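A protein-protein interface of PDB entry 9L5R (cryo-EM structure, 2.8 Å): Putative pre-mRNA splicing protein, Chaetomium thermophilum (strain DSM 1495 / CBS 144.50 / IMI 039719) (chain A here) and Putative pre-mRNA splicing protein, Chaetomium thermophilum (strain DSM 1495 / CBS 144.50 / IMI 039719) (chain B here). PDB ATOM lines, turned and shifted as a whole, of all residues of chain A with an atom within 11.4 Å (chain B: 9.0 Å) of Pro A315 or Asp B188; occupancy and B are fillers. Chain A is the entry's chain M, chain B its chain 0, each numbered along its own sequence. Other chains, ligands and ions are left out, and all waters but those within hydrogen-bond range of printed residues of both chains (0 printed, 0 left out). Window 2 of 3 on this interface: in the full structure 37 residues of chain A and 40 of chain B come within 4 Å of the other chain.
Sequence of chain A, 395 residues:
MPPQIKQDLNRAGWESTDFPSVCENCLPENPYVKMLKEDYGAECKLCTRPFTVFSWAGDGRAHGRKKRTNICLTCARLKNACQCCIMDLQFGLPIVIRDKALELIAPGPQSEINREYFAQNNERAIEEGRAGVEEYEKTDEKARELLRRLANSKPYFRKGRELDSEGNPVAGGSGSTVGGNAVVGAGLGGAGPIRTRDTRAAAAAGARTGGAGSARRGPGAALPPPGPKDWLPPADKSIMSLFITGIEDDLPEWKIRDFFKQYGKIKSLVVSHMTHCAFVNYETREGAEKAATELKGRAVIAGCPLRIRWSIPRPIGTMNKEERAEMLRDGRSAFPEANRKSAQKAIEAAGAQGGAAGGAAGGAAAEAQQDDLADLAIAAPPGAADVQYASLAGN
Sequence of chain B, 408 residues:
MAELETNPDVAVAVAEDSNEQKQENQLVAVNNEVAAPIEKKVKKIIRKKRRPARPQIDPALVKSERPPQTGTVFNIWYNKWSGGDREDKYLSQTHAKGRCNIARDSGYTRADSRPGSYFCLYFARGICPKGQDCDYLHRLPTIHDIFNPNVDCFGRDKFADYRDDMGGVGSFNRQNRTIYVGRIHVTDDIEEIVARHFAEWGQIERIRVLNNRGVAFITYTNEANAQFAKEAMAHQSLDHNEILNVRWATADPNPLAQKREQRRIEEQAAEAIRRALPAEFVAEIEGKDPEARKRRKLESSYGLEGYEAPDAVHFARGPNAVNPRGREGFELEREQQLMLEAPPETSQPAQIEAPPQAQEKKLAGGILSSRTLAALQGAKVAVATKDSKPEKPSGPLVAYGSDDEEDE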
ATOM      1  N   SER A 241      25.887   8.358 -37.019  1.00  0.00           N
ATOM      2  CA  SER A 241      26.531   7.256 -36.322  1.00  0.00           C
ATOM      3  C   SER A 241      27.300   6.370 -37.291  1.00  0.00           C
ATOM      4  O   SER A 241      26.759   5.932 -38.311  1.00  0.00           O
ATOM      5  CB  SER A 241      25.497   6.419 -35.570  1.00  0.00           C
ATOM      6  OG  SER A 241      24.709   7.241 -34.730  1.00  0.00           O
ATOM      7  N   LEU A 242      28.560   6.114 -36.961  1.00  0.00           N
ATOM      8  CA  LEU A 242      29.358   5.095 -37.622  1.00  0.00           C
ATOM      9  C   LEU A 242      29.226   3.784 -36.857  1.00  0.00           C
ATOM     10  O   LEU A 242      28.976   3.775 -35.650  1.00  0.00           O
ATOM     11  CB  LEU A 242      30.830   5.508 -37.707  1.00  0.00           C
ATOM     12  CG  LEU A 242      31.290   6.528 -38.759  1.00  0.00           C
ATOM     13  CD1 LEU A 242      30.829   7.954 -38.461  1.00  0.00           C
ATOM     14  CD2 LEU A 242      32.805   6.485 -38.915  1.00  0.00           C
ATOM     15  N   PHE A 243      29.398   2.677 -37.570  1.00  0.00           N
ATOM     16  CA  PHE A 243      29.190   1.346 -37.017  1.00  0.00           C
ATOM     17  C   PHE A 243      30.449   0.517 -37.218  1.00  0.00           C
ATOM     18  O   PHE A 243      30.911   0.354 -38.351  1.00  0.00           O
ATOM     19  CB  PHE A 243      27.992   0.676 -37.691  1.00  0.00           C
ATOM     20  CG  PHE A 243      27.546  -0.592 -37.029  1.00  0.00           C
ATOM     21  CD1 PHE A 243      27.080  -0.585 -35.728  1.00  0.00           C
ATOM     22  CD2 PHE A 243      27.583  -1.790 -37.716  1.00  0.00           C
ATOM     23  CE1 PHE A 243      26.665  -1.756 -35.124  1.00  0.00           C
ATOM     24  CE2 PHE A 243      27.169  -2.960 -37.120  1.00  0.00           C
ATOM     25  CZ  PHE A 243      26.709  -2.945 -35.821  1.00  0.00           C
ATOM     26  N   SER A 268      29.775  10.625 -28.534  1.00  0.00           N
ATOM     27  CA  SER A 268      29.701   9.429 -27.706  1.00  0.00           C
ATOM     28  C   SER A 268      30.288   8.254 -28.471  1.00  0.00           C
ATOM     29  O   SER A 268      30.378   8.269 -29.701  1.00  0.00           O
ATOM     30  CB  SER A 268      28.263   9.115 -27.292  1.00  0.00           C
ATOM     31  OG  SER A 268      27.495   8.744 -28.418  1.00  0.00           O
ATOM     32  N   VAL A 270      29.961   3.963 -28.064  1.00  0.00           N
ATOM     33  CA  VAL A 270      29.433   2.776 -27.406  1.00  0.00           C
ATOM     34  C   VAL A 270      30.147   1.567 -27.986  1.00  0.00           C
ATOM     35  O   VAL A 270      30.195   1.401 -29.209  1.00  0.00           O
ATOM     36  CB  VAL A 270      27.913   2.660 -27.601  1.00  0.00           C
ATOM     37  CG1 VAL A 270      27.361   1.490 -26.807  1.00  0.00           C
ATOM     38  CG2 VAL A 270      27.236   3.960 -27.216  1.00  0.00           C
ATOM     39  N   VAL A 271      30.715   0.736 -27.120  1.00  0.00           N
ATOM     40  CA  VAL A 271      31.400  -0.482 -27.536  1.00  0.00           C
ATOM     41  C   VAL A 271      30.864  -1.630 -26.699  1.00  0.00           C
ATOM     42  O   VAL A 271      30.907  -1.572 -25.464  1.00  0.00           O
ATOM     43  CB  VAL A 271      32.926  -0.372 -27.377  1.00  0.00           C
ATOM     44  CG1 VAL A 271      33.580  -1.729 -27.565  1.00  0.00           C
ATOM     45  CG2 VAL A 271      33.500   0.642 -28.351  1.00  0.00           C
ATOM     46  N   SER A 272      30.362  -2.670 -27.359  1.00  0.00           N
ATOM     47  CA  SER A 272      29.895  -3.871 -26.681  1.00  0.00           C
ATOM     48  C   SER A 272      30.782  -5.028 -27.113  1.00  0.00           C
ATOM     49  O   SER A 272      30.720  -5.468 -28.267  1.00  0.00           O
ATOM     50  CB  SER A 272      28.430  -4.154 -26.997  1.00  0.00           C
ATOM     51  OG  SER A 272      28.053  -5.431 -26.515  1.00  0.00           O
ATOM     52  N   THR A 275      28.715  -8.452 -27.952  1.00  0.00           N
ATOM     53  CA  THR A 275      28.200  -8.669 -29.296  1.00  0.00           C
ATOM     54  C   THR A 275      29.172  -8.219 -30.376  1.00  0.00           C
ATOM     55  O   THR A 275      28.802  -8.209 -31.554  1.00  0.00           O
ATOM     56  CB  THR A 275      26.868  -7.947 -29.476  1.00  0.00           C
ATOM     57  OG1 THR A 275      27.102  -6.535 -29.562  1.00  0.00           O
ATOM     58  CG2 THR A 275      25.932  -8.242 -28.310  1.00  0.00           C
ATOM     59  N   CYS A 277      30.298  -5.299 -31.192  1.00  0.00           N
ATOM     60  CA  CYS A 277      29.705  -4.199 -31.940  1.00  0.00           C
ATOM     61  C   CYS A 277      30.193  -2.861 -31.405  1.00  0.00           C
ATOM     62  O   CYS A 277      30.610  -2.749 -30.250  1.00  0.00           O
ATOM     63  CB  CYS A 277      28.175  -4.245 -31.868  1.00  0.00           C
ATOM     64  SG  CYS A 277      27.400  -5.572 -32.809  1.00  0.00           S
ATOM     65  N   ALA A 278      30.136  -1.833 -32.253  1.00  0.00           N
ATOM     66  CA  ALA A 278      30.336  -0.485 -31.739  1.00  0.00           C
ATOM     67  C   ALA A 278      29.546   0.529 -32.546  1.00  0.00           C
ATOM     68  O   ALA A 278      29.404   0.406 -33.762  1.00  0.00           O
ATOM     69  CB  ALA A 278      31.809  -0.072 -31.741  1.00  0.00           C
ATOM     70  N   PHE A 279      29.063   1.550 -31.848  1.00  0.00           N
ATOM     71  CA  PHE A 279      28.489   2.741 -32.452  1.00  0.00           C
ATOM     72  C   PHE A 279      29.347   3.938 -32.082  1.00  0.00           C
ATOM     73  O   PHE A 279      29.865   4.018 -30.964  1.00  0.00           O
ATOM     74  CB  PHE A 279      27.057   2.977 -31.979  1.00  0.00           C
ATOM     75  CG  PHE A 279      26.069   1.996 -32.521  1.00  0.00           C
ATOM     76  CD1 PHE A 279      25.832   0.802 -31.865  1.00  0.00           C
ATOM     77  CD2 PHE A 279      25.368   2.272 -33.682  1.00  0.00           C
ATOM     78  CE1 PHE A 279      24.918  -0.104 -32.360  1.00  0.00           C
ATOM     79  CE2 PHE A 279      24.450   1.370 -34.183  1.00  0.00           C
ATOM     80  CZ  PHE A 279      24.223   0.180 -33.519  1.00  0.00           C
ATOM     81  N   VAL A 280      29.516   4.859 -33.022  1.00  0.00           N
ATOM     82  CA  VAL A 280      30.240   6.101 -32.783  1.00  0.00           C
ATOM     83  C   VAL A 280      29.335   7.244 -33.204  1.00  0.00           C
ATOM     84  O   VAL A 280      28.945   7.331 -34.375  1.00  0.00           O
ATOM     85  CB  VAL A 280      31.569   6.162 -33.546  1.00  0.00           C
ATOM     86  CG1 VAL A 280      32.301   7.443 -33.204  1.00  0.00           C
ATOM     87  CG2 VAL A 280      32.429   4.971 -33.219  1.00  0.00           C
ATOM     88  N   ASN A 281      29.003   8.122 -32.266  1.00  0.00           N
ATOM     89  CA  ASN A 281      28.281   9.348 -32.570  1.00  0.00           C
ATOM     90  C   ASN A 281      29.286  10.487 -32.499  1.00  0.00           C
ATOM     91  O   ASN A 281      29.788  10.813 -31.420  1.00  0.00           O
ATOM     92  CB  ASN A 281      27.131   9.559 -31.590  1.00  0.00           C
ATOM     93  CG  ASN A 281      26.083   8.476 -31.687  1.00  0.00           C
ATOM     94  OD1 ASN A 281      25.405   8.339 -32.705  1.00  0.00           O
ATOM     95  ND2 ASN A 281      25.950   7.690 -30.630  1.00  0.00           N
ATOM     96  N   SER A 311      25.580   3.613 -40.296  1.00  0.00           N
ATOM     97  CA  SER A 311      24.373   2.908 -39.888  1.00  0.00           C
ATOM     98  C   SER A 311      23.584   3.786 -38.929  1.00  0.00           C
ATOM     99  O   SER A 311      24.129   4.692 -38.293  1.00  0.00           O
ATOM    100  CB  SER A 311      24.697   1.560 -39.234  1.00  0.00           C
ATOM    101  OG  SER A 311      23.516   0.808 -39.013  1.00  0.00           O
ATOM    102  N   ILE A 312      22.291   3.503 -38.843  1.00  0.00           N
ATOM    103  CA  ILE A 312      21.409   4.199 -37.898  1.00  0.00           C
ATOM    104  C   ILE A 312      21.747   3.750 -36.480  1.00  0.00           C
ATOM    105  O   ILE A 312      21.987   2.547 -36.263  1.00  0.00           O
ATOM    106  CB  ILE A 312      19.944   3.910 -38.241  1.00  0.00           C
ATOM    107  CG1 ILE A 312      19.708   4.108 -39.740  1.00  0.00           C
ATOM    108  CG2 ILE A 312      18.995   4.801 -37.455  1.00  0.00           C
ATOM    109  CD1 ILE A 312      18.339   3.663 -40.204  1.00  0.00           C
ATOM    110  N   PRO A 313      21.816   4.658 -35.502  1.00  0.00           N
ATOM    111  CA  PRO A 313      22.101   4.244 -34.116  1.00  0.00           C
ATOM    112  C   PRO A 313      21.002   3.354 -33.558  1.00  0.00           C
ATOM    113  O   PRO A 313      19.842   3.757 -33.450  1.00  0.00           O
ATOM    114  CB  PRO A 313      22.193   5.575 -33.361  1.00  0.00           C
ATOM    115  CG  PRO A 313      21.512   6.575 -34.244  1.00  0.00           C
ATOM    116  CD  PRO A 313      21.796   6.123 -35.638  1.00  0.00           C
ATOM    117  N   ARG A 314      21.385   2.133 -33.193  1.00  0.00           N
ATOM    118  CA  ARG A 314      20.472   1.078 -32.801  1.00  0.00           C
ATOM    119  C   ARG A 314      20.843   0.531 -31.429  1.00  0.00           C
ATOM    120  O   ARG A 314      22.032   0.403 -31.117  1.00  0.00           O
ATOM    121  CB  ARG A 314      20.503  -0.056 -33.837  1.00  0.00           C
ATOM    122  CG  ARG A 314      19.380  -1.071 -33.727  1.00  0.00           C
ATOM    123  CD  ARG A 314      19.523  -2.139 -34.795  1.00  0.00           C
ATOM    124  NE  ARG A 314      20.616  -3.059 -34.508  1.00  0.00           N
ATOM    125  CZ  ARG A 314      21.182  -3.849 -35.409  1.00  0.00           C
ATOM    126  NH1 ARG A 314      20.793  -3.844 -36.673  1.00  0.00           N
ATOM    127  NH2 ARG A 314      22.166  -4.661 -35.034  1.00  0.00           N
ATOM    128  N   PRO A 315      19.860   0.220 -30.582  1.00  0.00           N
ATOM    129  CA  PRO A 315      20.175  -0.416 -29.296  1.00  0.00           C
ATOM    130  C   PRO A 315      20.684  -1.835 -29.496  1.00  0.00           C
ATOM    131  O   PRO A 315      20.020  -2.669 -30.114  1.00  0.00           O
ATOM    132  CB  PRO A 315      18.833  -0.400 -28.552  1.00  0.00           C
ATOM    133  CG  PRO A 315      17.805  -0.221 -29.615  1.00  0.00           C
ATOM    134  CD  PRO A 315      18.451   0.634 -30.656  1.00  0.00           C
ATOM    135  N   ILE A 316      21.875  -2.101 -28.967  1.00  0.00           N
ATOM    136  CA  ILE A 316      22.452  -3.440 -29.014  1.00  0.00           C
ATOM    137  C   ILE A 316      21.684  -4.314 -28.026  1.00  0.00           C
ATOM    138  O   ILE A 316      21.824  -4.169 -26.809  1.00  0.00           O
ATOM    139  CB  ILE A 316      23.951  -3.420 -28.696  1.00  0.00           C
ATOM    140  CG1 ILE A 316      24.718  -2.728 -29.820  1.00  0.00           C
ATOM    141  CG2 ILE A 316      24.478  -4.829 -28.513  1.00  0.00           C
ATOM    142  CD1 ILE A 316      24.617  -3.444 -31.139  1.00  0.00           C
ATOM    143  N   GLY A 317      20.848  -5.206 -28.549  1.00  0.00           N
ATOM    144  CA  GLY A 317      20.083  -6.116 -27.727  1.00  0.00           C
ATOM    145  C   GLY A 317      20.848  -7.392 -27.434  1.00  0.00           C
ATOM    146  O   GLY A 317      22.055  -7.501 -27.653  1.00  0.00           O
ATOM    147  N   THR A 318      20.114  -8.376 -26.921  1.00  0.00           N
ATOM    148  CA  THR A 318      20.667  -9.701 -26.656  1.00  0.00           C
ATOM    149  C   THR A 318      20.645 -10.477 -27.966  1.00  0.00           C
ATOM    150  O   THR A 318      19.707 -11.219 -28.261  1.00  0.00           O
ATOM    151  CB  THR A 318      19.873 -10.414 -25.569  1.00  0.00           C
ATOM    152  OG1 THR A 318      18.502 -10.520 -25.970  1.00  0.00           O
ATOM    153  CG2 THR A 318      19.944  -9.633 -24.269  1.00  0.00           C
ATOM    154  N   MET A 319      21.692 -10.294 -28.767  1.00  0.00           N
ATOM    155  CA  MET A 319      21.747 -10.906 -30.083  1.00  0.00           C
ATOM    156  C   MET A 319      21.939 -12.415 -29.979  1.00  0.00           C
ATOM    157  O   MET A 319      22.341 -12.954 -28.944  1.00  0.00           O
ATOM    158  CB  MET A 319      22.875 -10.303 -30.921  1.00  0.00           C
ATOM    159  CG  MET A 319      22.951  -8.790 -30.880  1.00  0.00           C
ATOM    160  SD  MET A 319      24.260  -8.158 -31.947  1.00  0.00           S
ATOM    161  CE  MET A 319      23.453  -6.741 -32.679  1.00  0.00           C
ATOM    162  N   ASN A 320      21.623 -13.097 -31.075  1.00  0.00           N
ATOM    163  CA  ASN A 320      21.826 -14.531 -31.167  1.00  0.00           C
ATOM    164  C   ASN A 320      23.322 -14.840 -31.165  1.00  0.00           C
ATOM    165  O   ASN A 320      24.158 -14.010 -31.537  1.00  0.00           O
ATOM    166  CB  ASN A 320      21.161 -15.077 -32.435  1.00  0.00           C
ATOM    167  CG  ASN A 320      21.143 -16.600 -32.499  1.00  0.00           C
ATOM    168  OD1 ASN A 320      21.648 -17.287 -31.611  1.00  0.00           O
ATOM    169  ND2 ASN A 320      20.557 -17.131 -33.565  1.00  0.00           N
ATOM    170  N   GLU A 323      24.277 -14.631 -34.502  1.00  0.00           N
ATOM    171  CA  GLU A 323      24.390 -13.232 -34.909  1.00  0.00           C
ATOM    172  C   GLU A 323      25.746 -12.648 -34.536  1.00  0.00           C
ATOM    173  O   GLU A 323      26.413 -12.037 -35.379  1.00  0.00           O
ATOM    174  CB  GLU A 323      23.266 -12.401 -34.291  1.00  0.00           C
ATOM    175  CG  GLU A 323      21.966 -12.426 -35.076  1.00  0.00           C
ATOM    176  CD  GLU A 323      20.830 -11.744 -34.343  1.00  0.00           C
ATOM    177  OE1 GLU A 323      20.755 -11.872 -33.104  1.00  0.00           O
ATOM    178  OE2 GLU A 323      20.014 -11.070 -35.006  1.00  0.00           O
ATOM    179  N   MET A 327      28.854 -11.664 -36.908  1.00  0.00           N
ATOM    180  CA  MET A 327      29.390 -10.328 -36.680  1.00  0.00           C
ATOM    181  C   MET A 327      30.915 -10.381 -36.589  1.00  0.00           C
ATOM    182  O   MET A 327      31.624  -9.562 -37.196  1.00  0.00           O
ATOM    183  CB  MET A 327      28.774  -9.805 -35.381  1.00  0.00           C
ATOM    184  CG  MET A 327      29.005  -8.378 -34.990  1.00  0.00           C
ATOM    185  SD  MET A 327      28.156  -7.354 -36.203  1.00  0.00           S
ATOM    186  CE  MET A 327      29.041  -5.826 -36.053  1.00  0.00           C
ATOM    187  N   HIS B 185      16.544   4.516 -15.815  1.00  0.00           N
ATOM    188  CA  HIS B 185      15.316   4.461 -16.597  1.00  0.00           C
ATOM    189  C   HIS B 185      15.563   3.732 -17.913  1.00  0.00           C
ATOM    190  O   HIS B 185      16.413   4.137 -18.710  1.00  0.00           O
ATOM    191  CB  HIS B 185      14.802   5.876 -16.855  1.00  0.00           C
ATOM    192  CG  HIS B 185      13.369   5.930 -17.277  1.00  0.00           C
ATOM    193  ND1 HIS B 185      12.986   6.130 -18.586  1.00  0.00           N
ATOM    194  CD2 HIS B 185      12.224   5.807 -16.565  1.00  0.00           C
ATOM    195  CE1 HIS B 185      11.667   6.131 -18.662  1.00  0.00           C
ATOM    196  NE2 HIS B 185      11.181   5.937 -17.449  1.00  0.00           N
ATOM    197  N   VAL B 186      14.805   2.663 -18.142  1.00  0.00           N
ATOM    198  CA  VAL B 186      15.053   1.763 -19.265  1.00  0.00           C
ATOM    199  C   VAL B 186      14.500   2.395 -20.540  1.00  0.00           C
ATOM    200  O   VAL B 186      13.286   2.417 -20.759  1.00  0.00           O
ATOM    201  CB  VAL B 186      14.434   0.382 -19.022  1.00  0.00           C
ATOM    202  CG1 VAL B 186      14.652  -0.516 -20.226  1.00  0.00           C
ATOM    203  CG2 VAL B 186      15.019  -0.250 -17.776  1.00  0.00           C
ATOM    204  N   THR B 187      15.392   2.924 -21.377  1.00  0.00           N
ATOM    205  CA  THR B 187      15.045   3.346 -22.730  1.00  0.00           C
ATOM    206  C   THR B 187      16.007   2.698 -23.717  1.00  0.00           C
ATOM    207  O   THR B 187      16.766   1.797 -23.348  1.00  0.00           O
ATOM    208  CB  THR B 187      15.079   4.871 -22.880  1.00  0.00           C
ATOM    209  OG1 THR B 187      16.412   5.353 -22.665  1.00  0.00           O
ATOM    210  CG2 THR B 187      14.126   5.547 -21.902  1.00  0.00           C
ATOM    211  N   ASP B 188      15.980   3.134 -24.975  1.00  0.00           N
ATOM    212  CA  ASP B 188      16.850   2.558 -25.990  1.00  0.00           C
ATOM    213  C   ASP B 188      18.176   3.292 -26.138  1.00  0.00           C
ATOM    214  O   ASP B 188      19.146   2.695 -26.618  1.00  0.00           O
ATOM    215  CB  ASP B 188      16.138   2.529 -27.344  1.00  0.00           C
ATOM    216  CG  ASP B 188      14.994   1.541 -27.377  1.00  0.00           C
ATOM    217  OD1 ASP B 188      15.065   0.528 -26.649  1.00  0.00           O
ATOM    218  OD2 ASP B 188      14.026   1.773 -28.130  1.00  0.00           O
ATOM    219  N   ASP B 189      18.247   4.561 -25.740  1.00  0.00           N
ATOM    220  CA  ASP B 189      19.473   5.341 -25.836  1.00  0.00           C
ATOM    221  C   ASP B 189      20.321   5.255 -24.572  1.00  0.00           C
ATOM    222  O   ASP B 189      21.229   6.080 -24.390  1.00  0.00           O
ATOM    223  CB  ASP B 189      19.144   6.801 -26.149  1.00  0.00           C
ATOM    224  CG  ASP B 189      18.077   7.366 -25.233  1.00  0.00           C
ATOM    225  OD1 ASP B 189      17.294   6.570 -24.674  1.00  0.00           O
ATOM    226  OD2 ASP B 189      18.020   8.604 -25.072  1.00  0.00           O
ATOM    227  N   ILE B 190      20.041   4.279 -23.703  1.00  0.00           N
ATOM    228  CA  ILE B 190      20.705   4.209 -22.404  1.00  0.00           C
ATOM    229  C   ILE B 190      22.192   3.942 -22.571  1.00  0.00           C
ATOM    230  O   ILE B 190      23.013   4.469 -21.814  1.00  0.00           O
ATOM    231  CB  ILE B 190      20.036   3.152 -21.504  1.00  0.00           C
ATOM    232  CG1 ILE B 190      19.909   1.806 -22.215  1.00  0.00           C
ATOM    233  CG2 ILE B 190      18.681   3.632 -21.052  1.00  0.00           C
ATOM    234  CD1 ILE B 190      19.448   0.694 -21.307  1.00  0.00           C
ATOM    235  N   GLU B 191      22.565   3.138 -23.569  1.00  0.00           N
ATOM    236  CA  GLU B 191      23.978   2.861 -23.803  1.00  0.00           C
ATOM    237  C   GLU B 191      24.718   4.117 -24.241  1.00  0.00           C
ATOM    238  O   GLU B 191      25.829   4.383 -23.769  1.00  0.00           O
ATOM    239  CB  GLU B 191      24.120   1.750 -24.838  1.00  0.00           C
ATOM    240  CG  GLU B 191      23.150   0.604 -24.612  1.00  0.00           C
ATOM    241  CD  GLU B 191      23.499  -0.624 -25.416  1.00  0.00           C
ATOM    242  OE1 GLU B 191      24.475  -0.569 -26.194  1.00  0.00           O
ATOM    243  OE2 GLU B 191      22.792  -1.644 -25.274  1.00  0.00           O
ATOM    244  N   GLU B 192      24.096   4.918 -25.110  1.00  0.00           N
ATOM    245  CA  GLU B 192      24.690   6.184 -25.527  1.00  0.00           C
ATOM    246  C   GLU B 192      24.837   7.145 -24.353  1.00  0.00           C
ATOM    247  O   GLU B 192      25.874   7.803 -24.204  1.00  0.00           O
ATOM    248  CB  GLU B 192      23.838   6.812 -26.629  1.00  0.00           C
ATOM    249  CG  GLU B 192      24.552   7.854 -27.468  1.00  0.00           C
ATOM    250  CD  GLU B 192      24.400   9.260 -26.920  1.00  0.00           C
ATOM    251  OE1 GLU B 192      23.543   9.466 -26.036  1.00  0.00           O
ATOM    252  OE2 GLU B 192      25.131  10.161 -27.380  1.00  0.00           O
ATOM    253  N   ILE B 193      23.810   7.225 -23.503  1.00  0.00           N
ATOM    254  CA  ILE B 193      23.843   8.148 -22.371  1.00  0.00           C
ATOM    255  C   ILE B 193      24.912   7.736 -21.359  1.00  0.00           C
ATOM    256  O   ILE B 193      25.686   8.578 -20.873  1.00  0.00           O
ATOM    257  CB  ILE B 193      22.445   8.227 -21.733  1.00  0.00           C
ATOM    258  CG1 ILE B 193      21.452   8.836 -22.723  1.00  0.00           C
ATOM    259  CG2 ILE B 193      22.475   9.051 -20.472  1.00  0.00           C
ATOM    260  CD1 ILE B 193      20.011   8.600 -22.356  1.00  0.00           C
ATOM    261  N   VAL B 194      24.976   6.438 -21.036  1.00  0.00           N
ATOM    262  CA  VAL B 194      25.985   5.920 -20.116  1.00  0.00           C
ATOM    263  C   VAL B 194      27.384   6.146 -20.668  1.00  0.00           C
ATOM    264  O   VAL B 194      28.283   6.601 -19.947  1.00  0.00           O
ATOM    265  CB  VAL B 194      25.719   4.430 -19.822  1.00  0.00           C
ATOM    266  CG1 VAL B 194      26.884   3.808 -19.091  1.00  0.00           C
ATOM    267  CG2 VAL B 194      24.475   4.280 -18.972  1.00  0.00           C
ATOM    268  N   VAL B 209      26.486  -2.475 -20.236  1.00  0.00           N
ATOM    269  CA  VAL B 209      25.163  -1.978 -19.743  1.00  0.00           C
ATOM    270  C   VAL B 209      24.067  -3.016 -20.024  1.00  0.00           C
ATOM    271  O   VAL B 209      23.880  -3.383 -21.206  1.00  0.00           O
ATOM    272  CB  VAL B 209      24.839  -0.579 -20.314  1.00  0.00           C
ATOM    273  CG1 VAL B 209      25.398  -0.371 -21.713  1.00  0.00           C
ATOM    274  CG2 VAL B 209      23.361  -0.222 -20.245  1.00  0.00           C
ATOM    275  N   ASN B 211      20.028  -4.086 -20.069  1.00  0.00           N
ATOM    276  CA  ASN B 211      18.809  -3.263 -20.306  1.00  0.00           C
ATOM    277  C   ASN B 211      17.638  -3.834 -19.502  1.00  0.00           C
ATOM    278  O   ASN B 211      16.765  -3.039 -19.111  1.00  0.00           O
ATOM    279  CB  ASN B 211      18.478  -3.166 -21.799  1.00  0.00           C
ATOM    280  CG  ASN B 211      19.701  -3.238 -22.691  1.00  0.00           C
ATOM    281  OD1 ASN B 211      20.620  -2.431 -22.565  1.00  0.00           O
ATOM    282  ND2 ASN B 211      19.724  -4.205 -23.593  1.00  0.00           N
ATOM    283  N   HIS B 240      17.330  11.549 -17.931  1.00  0.00           N
ATOM    284  CA  HIS B 240      16.104  11.605 -17.150  1.00  0.00           C
ATOM    285  C   HIS B 240      16.420  11.880 -15.683  1.00  0.00           C
ATOM    286  O   HIS B 240      17.523  11.620 -15.199  1.00  0.00           O
ATOM    287  CB  HIS B 240      15.319  10.299 -17.281  1.00  0.00           C
ATOM    288  CG  HIS B 240      15.338   9.725 -18.662  1.00  0.00           C
ATOM    289  ND1 HIS B 240      14.783  10.375 -19.742  1.00  0.00           N
ATOM    290  CD2 HIS B 240      15.846   8.566 -19.139  1.00  0.00           C
ATOM    291  CE1 HIS B 240      14.949   9.639 -20.826  1.00  0.00           C
ATOM    292  NE2 HIS B 240      15.590   8.535 -20.487  1.00  0.00           N
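Of the 25 printed residues of chain A, 5 touch a printed residue of chain B. Hydrophobic or aromatic side chains of chain A that line the printed part of chain B: Val A270, Pro A315 and Ile A316. Of the 13 printed residues of chain B, 4 touch a printed residue of chain A. Among the printed residues, no Asp or Glu carboxylate lies within 4 Å of a Lys or Arg side-chain nitrogen of the other chain.
Pro A315 touches just one residue of chain B: Asp B188 (3.7 Å). Asp B188 touches one residue of chain A. No residue of chain A comes within 4 Å of Asp B189. Ile B190 touches none of the printed residues of chain A. Of the printed residues of chain A, Asn B211 touches Ile A316. Printed residues of chain B within 4 Å of Asn A281: Glu B192. Printed residues of chain B within 4 Å of Ser A268: Glu B192 (2.9 Å). Of the printed residues of chain A, Glu B192 touches Ser A268, Val A270 and Asn A281. Printed residues of chain B within 4 Å of Val A270: Glu B191 and Glu B192. Glu A323 touches none of the printed residues of chain B. Leu A242 touches none of the printed residues of chain B. The nearest residue of chain B that does not touch Pro A315 is Glu B191 (4.7 Å).
The side-chain hydroxyl (OG) of Ser A268 sits at hydrogen-bond distance from the side-chain carboxylate (OE2) of Glu B192 (2.9 Å). The side-chain carboxylate (OE2) of Glu B191 sits close to the backbone carbonyl oxygen (O) of Ile A316, 3.1 Å away.
The side-chain hydroxyl (OG) of Ser A241 sits at hydrogen-bond distance from the side-chain amide oxygen (OD1) of Asn A281 (2.4 Å). The backbone carbonyl oxygen (O) of Val A270 sits at hydrogen-bond distance from the backbone NH (N) of Phe A279 (2.9 Å). O of Asn A281 sits at hydrogen-bond distance from N of Ser A268, at 2.9 Å.
Glu B191 touches Val A270 (OE1 to CG1, 3.6 Å). Val A270 touches Glu B192. Glu B192 touches Asn A281 (CG to ND2, 3.5 Å). CB of Pro A315 touches O of Asp B188, 3.7 Å away. Asn B211 touches Ile A316.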
